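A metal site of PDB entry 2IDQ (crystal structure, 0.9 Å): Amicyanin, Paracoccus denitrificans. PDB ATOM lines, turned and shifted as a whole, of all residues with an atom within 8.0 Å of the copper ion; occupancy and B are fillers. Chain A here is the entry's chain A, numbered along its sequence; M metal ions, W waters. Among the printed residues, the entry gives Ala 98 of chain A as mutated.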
ATOM      1  N   ILE A  25       8.764  -7.464  -4.984  1.00  0.00           N
ATOM      2  CA  ILE A  25       8.504  -7.624  -6.399  1.00  0.00           C
ATOM      3  C   ILE A  25       8.524  -9.102  -6.709  1.00  0.00           C
ATOM      4  O   ILE A  25       9.507  -9.811  -6.415  1.00  0.00           O
ATOM      5  CB  ILE A  25       9.563  -6.877  -7.242  1.00  0.00           C
ATOM      6  CG1 ILE A  25       9.797  -5.445  -6.771  1.00  0.00           C
ATOM      7  CG2 ILE A  25       9.142  -6.909  -8.674  1.00  0.00           C
ATOM      8  CD1 ILE A  25      10.931  -4.735  -7.440  1.00  0.00           C
ATOM      9  N   MET A  28       6.467 -10.578 -11.701  1.00  0.00           N
ATOM     10  CA  MET A  28       6.512  -9.462 -12.649  1.00  0.00           C
ATOM     11  C   MET A  28       5.587  -8.321 -12.205  1.00  0.00           C
ATOM     12  O   MET A  28       5.077  -7.530 -13.017  1.00  0.00           O
ATOM     13  CB  MET A  28       6.231  -9.854 -14.104  1.00  0.00           C
ATOM     14  CG  MET A  28       6.955 -11.124 -14.580  1.00  0.00           C
ATOM     15  SD  MET A  28       8.735 -10.896 -14.801  1.00  0.00           S
ATOM     16  CE  MET A  28       8.641  -9.762 -16.192  1.00  0.00           C
ATOM     17  N   LYS A  29       5.396  -8.133 -10.900  1.00  0.00           N
ATOM     18  CA  LYS A  29       4.513  -7.074 -10.408  1.00  0.00           C
ATOM     19  C   LYS A  29       5.044  -6.568  -9.075  1.00  0.00           C
ATOM     20  O   LYS A  29       5.723  -7.305  -8.350  1.00  0.00           O
ATOM     21  CB  LYS A  29       3.041  -7.530 -10.299  1.00  0.00           C
ATOM     22  CG  LYS A  29       2.405  -8.065 -11.499  1.00  0.00           C
ATOM     23  CD  LYS A  29       1.104  -8.803 -11.391  1.00  0.00           C
ATOM     24  CE  LYS A  29       1.146 -10.225 -11.971  1.00  0.00           C
ATOM     25  NZ  LYS A  29       0.181 -10.996 -11.127  1.00  0.00           N
ATOM     26  N   TYR A  30       4.702  -5.350  -8.751  1.00  0.00           N
ATOM     27  CA  TYR A  30       4.924  -4.870  -7.386  1.00  0.00           C
ATOM     28  C   TYR A  30       3.815  -5.417  -6.513  1.00  0.00           C
ATOM     29  O   TYR A  30       2.626  -5.229  -6.816  1.00  0.00           O
ATOM     30  CB  TYR A  30       4.928  -3.333  -7.375  1.00  0.00           C
ATOM     31  CG  TYR A  30       5.948  -2.734  -8.301  1.00  0.00           C
ATOM     32  CD1 TYR A  30       7.313  -2.826  -8.019  1.00  0.00           C
ATOM     33  CD2 TYR A  30       5.578  -2.101  -9.473  1.00  0.00           C
ATOM     34  CE1 TYR A  30       8.250  -2.317  -8.875  1.00  0.00           C
ATOM     35  CE2 TYR A  30       6.527  -1.584 -10.328  1.00  0.00           C
ATOM     36  CZ  TYR A  30       7.860  -1.695 -10.025  1.00  0.00           C
ATOM     37  OH  TYR A  30       8.747  -1.084 -10.899  1.00  0.00           O
ATOM     38  N   ASN A  47      13.540  -7.290  -4.835  1.00  0.00           N
ATOM     39  CA  ASN A  47      13.196  -8.189  -5.922  1.00  0.00           C
ATOM     40  C   ASN A  47      13.250  -9.635  -5.396  1.00  0.00           C
ATOM     41  O   ASN A  47      14.298 -10.080  -4.944  1.00  0.00           O
ATOM     42  CB  ASN A  47      14.154  -8.026  -7.081  1.00  0.00           C
ATOM     43  CG  ASN A  47      13.697  -8.842  -8.274  1.00  0.00           C
ATOM     44  OD1 ASN A  47      12.616  -9.474  -8.256  1.00  0.00           O
ATOM     45  ND2 ASN A  47      14.461  -8.824  -9.329  1.00  0.00           N
ATOM     46  N   GLU A  49      12.389 -12.283  -7.311  1.00  0.00           N
ATOM     47  CA  GLU A  49      12.553 -13.285  -8.351  1.00  0.00           C
ATOM     48  C   GLU A  49      13.722 -13.032  -9.228  1.00  0.00           C
ATOM     49  O   GLU A  49      14.410 -12.056  -9.149  1.00  0.00           O
ATOM     50  CB  GLU A  49      11.250 -13.419  -9.142  1.00  0.00           C
ATOM     51  CG  GLU A  49      10.953 -12.101  -9.800  1.00  0.00           C
ATOM     52  CD  GLU A  49       9.683 -12.246 -10.659  1.00  0.00           C
ATOM     53  OE1 GLU A  49       9.183 -13.339 -10.819  1.00  0.00           O
ATOM     54  OE2 GLU A  49       9.157 -11.232 -11.173  1.00  0.00           O
ATOM     55  N   MET A  51      14.177 -12.701 -12.523  1.00  0.00           N
ATOM     56  CA  MET A  51      14.154 -11.676 -13.554  1.00  0.00           C
ATOM     57  C   MET A  51      14.462 -10.312 -12.928  1.00  0.00           C
ATOM     58  O   MET A  51      13.811  -9.938 -11.957  1.00  0.00           O
ATOM     59  CB  MET A  51      12.799 -11.587 -14.193  1.00  0.00           C
ATOM     60  CG  MET A  51      12.574 -10.657 -15.304  1.00  0.00           C
ATOM     61  SD  MET A  51      13.779 -10.677 -16.597  1.00  0.00           S
ATOM     62  CE  MET A  51      14.082 -12.446 -16.857  1.00  0.00           C
ATOM     63  N   PRO A  52      15.415  -9.568 -13.463  1.00  0.00           N
ATOM     64  CA  PRO A  52      15.715  -8.252 -12.860  1.00  0.00           C
ATOM     65  C   PRO A  52      14.612  -7.249 -13.066  1.00  0.00           C
ATOM     66  O   PRO A  52      13.938  -7.201 -14.112  1.00  0.00           O
ATOM     67  CB  PRO A  52      16.992  -7.834 -13.611  1.00  0.00           C
ATOM     68  CG  PRO A  52      17.629  -9.128 -14.084  1.00  0.00           C
ATOM     69  CD  PRO A  52      16.427  -9.929 -14.470  1.00  0.00           C
ATOM     70  N   HIS A  53      14.428  -6.405 -12.055  1.00  0.00           N
ATOM     71  CA  HIS A  53      13.423  -5.379 -12.010  1.00  0.00           C
ATOM     72  C   HIS A  53      14.005  -4.101 -11.428  1.00  0.00           C
ATOM     73  O   HIS A  53      14.950  -4.173 -10.630  1.00  0.00           O
ATOM     74  CB  HIS A  53      12.247  -5.787 -11.148  1.00  0.00           C
ATOM     75  CG  HIS A  53      11.523  -7.005 -11.653  1.00  0.00           C
ATOM     76  ND1 HIS A  53      10.856  -7.005 -12.875  1.00  0.00           N
ATOM     77  CD2 HIS A  53      11.344  -8.202 -11.062  1.00  0.00           C
ATOM     78  CE1 HIS A  53      10.305  -8.207 -12.990  1.00  0.00           C
ATOM     79  NE2 HIS A  53      10.586  -8.948 -11.919  1.00  0.00           N
ATOM     80  N   ASN A  54      13.374  -2.967 -11.675  1.00  0.00           N
ATOM     81  CA  ASN A  54      13.758  -1.723 -11.010  1.00  0.00           C
ATOM     82  C   ASN A  54      12.482  -0.963 -10.651  1.00  0.00           C
ATOM     83  O   ASN A  54      11.368  -1.460 -10.786  1.00  0.00           O
ATOM     84  CB  ASN A  54      14.719  -0.883 -11.838  1.00  0.00           C
ATOM     85  CG  ASN A  54      14.077  -0.192 -12.991  1.00  0.00           C
ATOM     86  OD1 ASN A  54      13.010  -0.587 -13.428  1.00  0.00           O
ATOM     87  ND2 ASN A  54      14.768   0.828 -13.508  1.00  0.00           N
ATOM     88  N   VAL A  55      12.696   0.288 -10.217  1.00  0.00           N
ATOM     89  CA  VAL A  55      11.652   1.288 -10.116  1.00  0.00           C
ATOM     90  C   VAL A  55      12.124   2.506 -10.905  1.00  0.00           C
ATOM     91  O   VAL A  55      13.300   2.870 -10.840  1.00  0.00           O
ATOM     92  CB  VAL A  55      11.296   1.662  -8.672  1.00  0.00           C
ATOM     93  CG1 VAL A  55      10.706   0.442  -7.981  1.00  0.00           C
ATOM     94  CG2 VAL A  55      12.454   2.243  -7.888  1.00  0.00           C
ATOM     95  N   MET A  71      18.813  -1.825 -11.855  1.00  0.00           N
ATOM     96  CA  MET A  71      18.203  -3.139 -11.986  1.00  0.00           C
ATOM     97  C   MET A  71      18.635  -4.006 -10.805  1.00  0.00           C
ATOM     98  O   MET A  71      19.809  -4.170 -10.522  1.00  0.00           O
ATOM     99  CB  MET A  71      18.628  -3.763 -13.315  1.00  0.00           C
ATOM    100  CG  MET A  71      18.193  -3.012 -14.535  1.00  0.00           C
ATOM    101  SD  MET A  71      16.459  -2.550 -14.624  1.00  0.00           S
ATOM    102  CE  MET A  71      15.691  -4.162 -14.512  1.00  0.00           C
ATOM    103  N   MET A  72      17.683  -4.546 -10.109  1.00  0.00           N
ATOM    104  CA  MET A  72      17.875  -5.417  -8.980  1.00  0.00           C
ATOM    105  C   MET A  72      17.807  -6.860  -9.425  1.00  0.00           C
ATOM    106  O   MET A  72      16.805  -7.278 -10.030  1.00  0.00           O
ATOM    107  CB  MET A  72      16.733  -5.199  -7.944  1.00  0.00           C
ATOM    108  CG  MET A  72      16.778  -3.956  -7.114  1.00  0.00           C
ATOM    109  SD  MET A  72      15.295  -3.669  -6.106  1.00  0.00           S
ATOM    110  CE  MET A  72      14.235  -2.928  -7.336  1.00  0.00           C
ATOM    111  N   HIS A  91       7.183   2.809 -12.548  1.00  0.00           N
ATOM    112  CA  HIS A  91       7.038   1.564 -13.298  1.00  0.00           C
ATOM    113  C   HIS A  91       8.376   0.886 -13.358  1.00  0.00           C
ATOM    114  O   HIS A  91       9.410   1.441 -12.981  1.00  0.00           O
ATOM    115  CB  HIS A  91       6.451   1.837 -14.686  1.00  0.00           C
ATOM    116  CG  HIS A  91       7.408   2.553 -15.593  1.00  0.00           C
ATOM    117  ND1 HIS A  91       7.570   3.907 -15.592  1.00  0.00           N
ATOM    118  CD2 HIS A  91       8.309   2.060 -16.481  1.00  0.00           C
ATOM    119  CE1 HIS A  91       8.505   4.230 -16.473  1.00  0.00           C
ATOM    120  NE2 HIS A  91       8.966   3.136 -17.034  1.00  0.00           N
ATOM    121  N   CYS A  92       8.378  -0.339 -13.918  1.00  0.00           N
ATOM    122  CA  CYS A  92       9.630  -1.074 -14.107  1.00  0.00           C
ATOM    123  C   CYS A  92      10.140  -0.804 -15.522  1.00  0.00           C
ATOM    124  O   CYS A  92       9.414  -0.981 -16.496  1.00  0.00           O
ATOM    125  CB  CYS A  92       9.374  -2.572 -13.903  1.00  0.00           C
ATOM    126  SG  CYS A  92      10.947  -3.456 -14.180  1.00  0.00           S
ATOM    127  N   THR A  93      11.352  -0.326 -15.656  1.00  0.00           N
ATOM    128  CA  THR A  93      11.874   0.124 -16.929  1.00  0.00           C
ATOM    129  C   THR A  93      11.687  -0.902 -18.065  1.00  0.00           C
ATOM    130  O   THR A  93      11.096  -0.535 -19.081  1.00  0.00           O
ATOM    131  CB  THR A  93      13.351   0.578 -16.820  1.00  0.00           C
ATOM    132  OG1 THR A  93      13.394   1.675 -15.926  1.00  0.00           O
ATOM    133  CG2 THR A  93      13.919   0.954 -18.146  1.00  0.00           C
ATOM    134  N   PRO A  94      12.150  -2.139 -17.914  1.00  0.00           N
ATOM    135  CA  PRO A  94      11.963  -3.107 -19.008  1.00  0.00           C
ATOM    136  C   PRO A  94      10.547  -3.642 -19.100  1.00  0.00           C
ATOM    137  O   PRO A  94      10.187  -4.204 -20.151  1.00  0.00           O
ATOM    138  CB  PRO A  94      12.930  -4.249 -18.643  1.00  0.00           C
ATOM    139  CG  PRO A  94      13.085  -4.158 -17.154  1.00  0.00           C
ATOM    140  CD  PRO A  94      13.076  -2.665 -16.886  1.00  0.00           C
ATOM    141  N   HIS A  95       9.764  -3.503 -18.049  1.00  0.00           N
ATOM    142  CA  HIS A  95       8.453  -4.106 -17.877  1.00  0.00           C
ATOM    143  C   HIS A  95       7.433  -3.025 -17.539  1.00  0.00           C
ATOM    144  O   HIS A  95       6.849  -3.012 -16.438  1.00  0.00           O
ATOM    145  CB  HIS A  95       8.478  -5.156 -16.788  1.00  0.00           C
ATOM    146  CG  HIS A  95       9.558  -6.184 -16.972  1.00  0.00           C
ATOM    147  ND1 HIS A  95      10.417  -6.505 -15.954  1.00  0.00           N
ATOM    148  CD2 HIS A  95       9.840  -6.957 -18.076  1.00  0.00           C
ATOM    149  CE1 HIS A  95      11.245  -7.416 -16.456  1.00  0.00           C
ATOM    150  NE2 HIS A  95      10.928  -7.695 -17.694  1.00  0.00           N
ATOM    151  N   PRO A  96       7.156  -2.082 -18.466  1.00  0.00           N
ATOM    152  CA  PRO A  96       6.346  -0.925 -18.078  1.00  0.00           C
ATOM    153  C   PRO A  96       4.877  -1.212 -17.843  1.00  0.00           C
ATOM    154  O   PRO A  96       4.156  -0.348 -17.417  1.00  0.00           O
ATOM    155  CB  PRO A  96       6.600   0.059 -19.220  1.00  0.00           C
ATOM    156  CG  PRO A  96       6.961  -0.810 -20.391  1.00  0.00           C
ATOM    157  CD  PRO A  96       7.773  -1.897 -19.782  1.00  0.00           C
ATOM    158  N   PHE A  97       4.445  -2.449 -18.159  1.00  0.00           N
ATOM    159  CA  PHE A  97       3.134  -2.913 -17.713  1.00  0.00           C
ATOM    160  C   PHE A  97       3.043  -3.006 -16.202  1.00  0.00           C
ATOM    161  O   PHE A  97       1.914  -3.116 -15.673  1.00  0.00           O
ATOM    162  CB  PHE A  97       2.796  -4.251 -18.387  1.00  0.00           C
ATOM    163  CG  PHE A  97       3.862  -5.323 -18.199  1.00  0.00           C
ATOM    164  CD1 PHE A  97       3.983  -6.043 -17.024  1.00  0.00           C
ATOM    165  CD2 PHE A  97       4.775  -5.600 -19.203  1.00  0.00           C
ATOM    166  CE1 PHE A  97       4.979  -6.964 -16.820  1.00  0.00           C
ATOM    167  CE2 PHE A  97       5.767  -6.535 -19.033  1.00  0.00           C
ATOM    168  CZ  PHE A  97       5.881  -7.211 -17.819  1.00  0.00           C
ATOM    169  N   ALA A  98       4.155  -3.062 -15.496  1.00  0.00           N
ATOM    170  CA  ALA A  98       4.185  -3.152 -14.031  1.00  0.00           C
ATOM    171  C   ALA A  98       4.355  -1.736 -13.481  1.00  0.00           C
ATOM    172  O   ALA A  98       5.374  -1.115 -13.660  1.00  0.00           O
ATOM    173  CB  ALA A  98       5.352  -4.029 -13.593  1.00  0.00           C
HETATM  174 CU    CU M   1      10.629  -5.572 -14.182  1.00  0.00          CU
HETATM  175  O   HOH W   1       8.326  -5.848 -13.514  1.00  0.00           O
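Merely in contact with the copper ion: Pro 52 (3.7 Å). Four residues have an atom within 4 Å of the copper ion: Pro 52, His 53, Cys 92 and His 95. Along chain A the residues within 4 Å of the copper ion span positions 52 to 95.
N of Cys 92 sits at hydrogen-bond distance from OH of Tyr 30 (3.1 Å). The backbone NH of Cys 92 is in hydrogen-bond range of the backbone carbonyl oxygen of Ala 98 (3.1 Å). A ring nitrogen (NE2) of His 53 is in hydrogen-bond range of the side-chain carboxylate (OE2) of Glu 49, at 2.8 Å. O of Met 51 lies close to NE2 of His 53 (3.4 Å). The side-chain sulfur (SG) of Cys 92 sits close to the backbone NH (N) of Asn 54 (3.5 Å). The backbone carbonyl oxygen (O) of His 53 lies within hydrogen-bond range of the backbone NH (N) of Met 72 (2.8 Å).
ND1 of His 53 is bound to the copper ion (2.0 Å). The copper ion is bound by ND1 of His 95, at 2.0 Å. The copper ion is bound by the side-chain sulfur (SG) of Cys 92, at 2.1 Å. The copper ion is bound by water W1 (2.4 Å). The copper ion has four donor atoms within binding distance.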
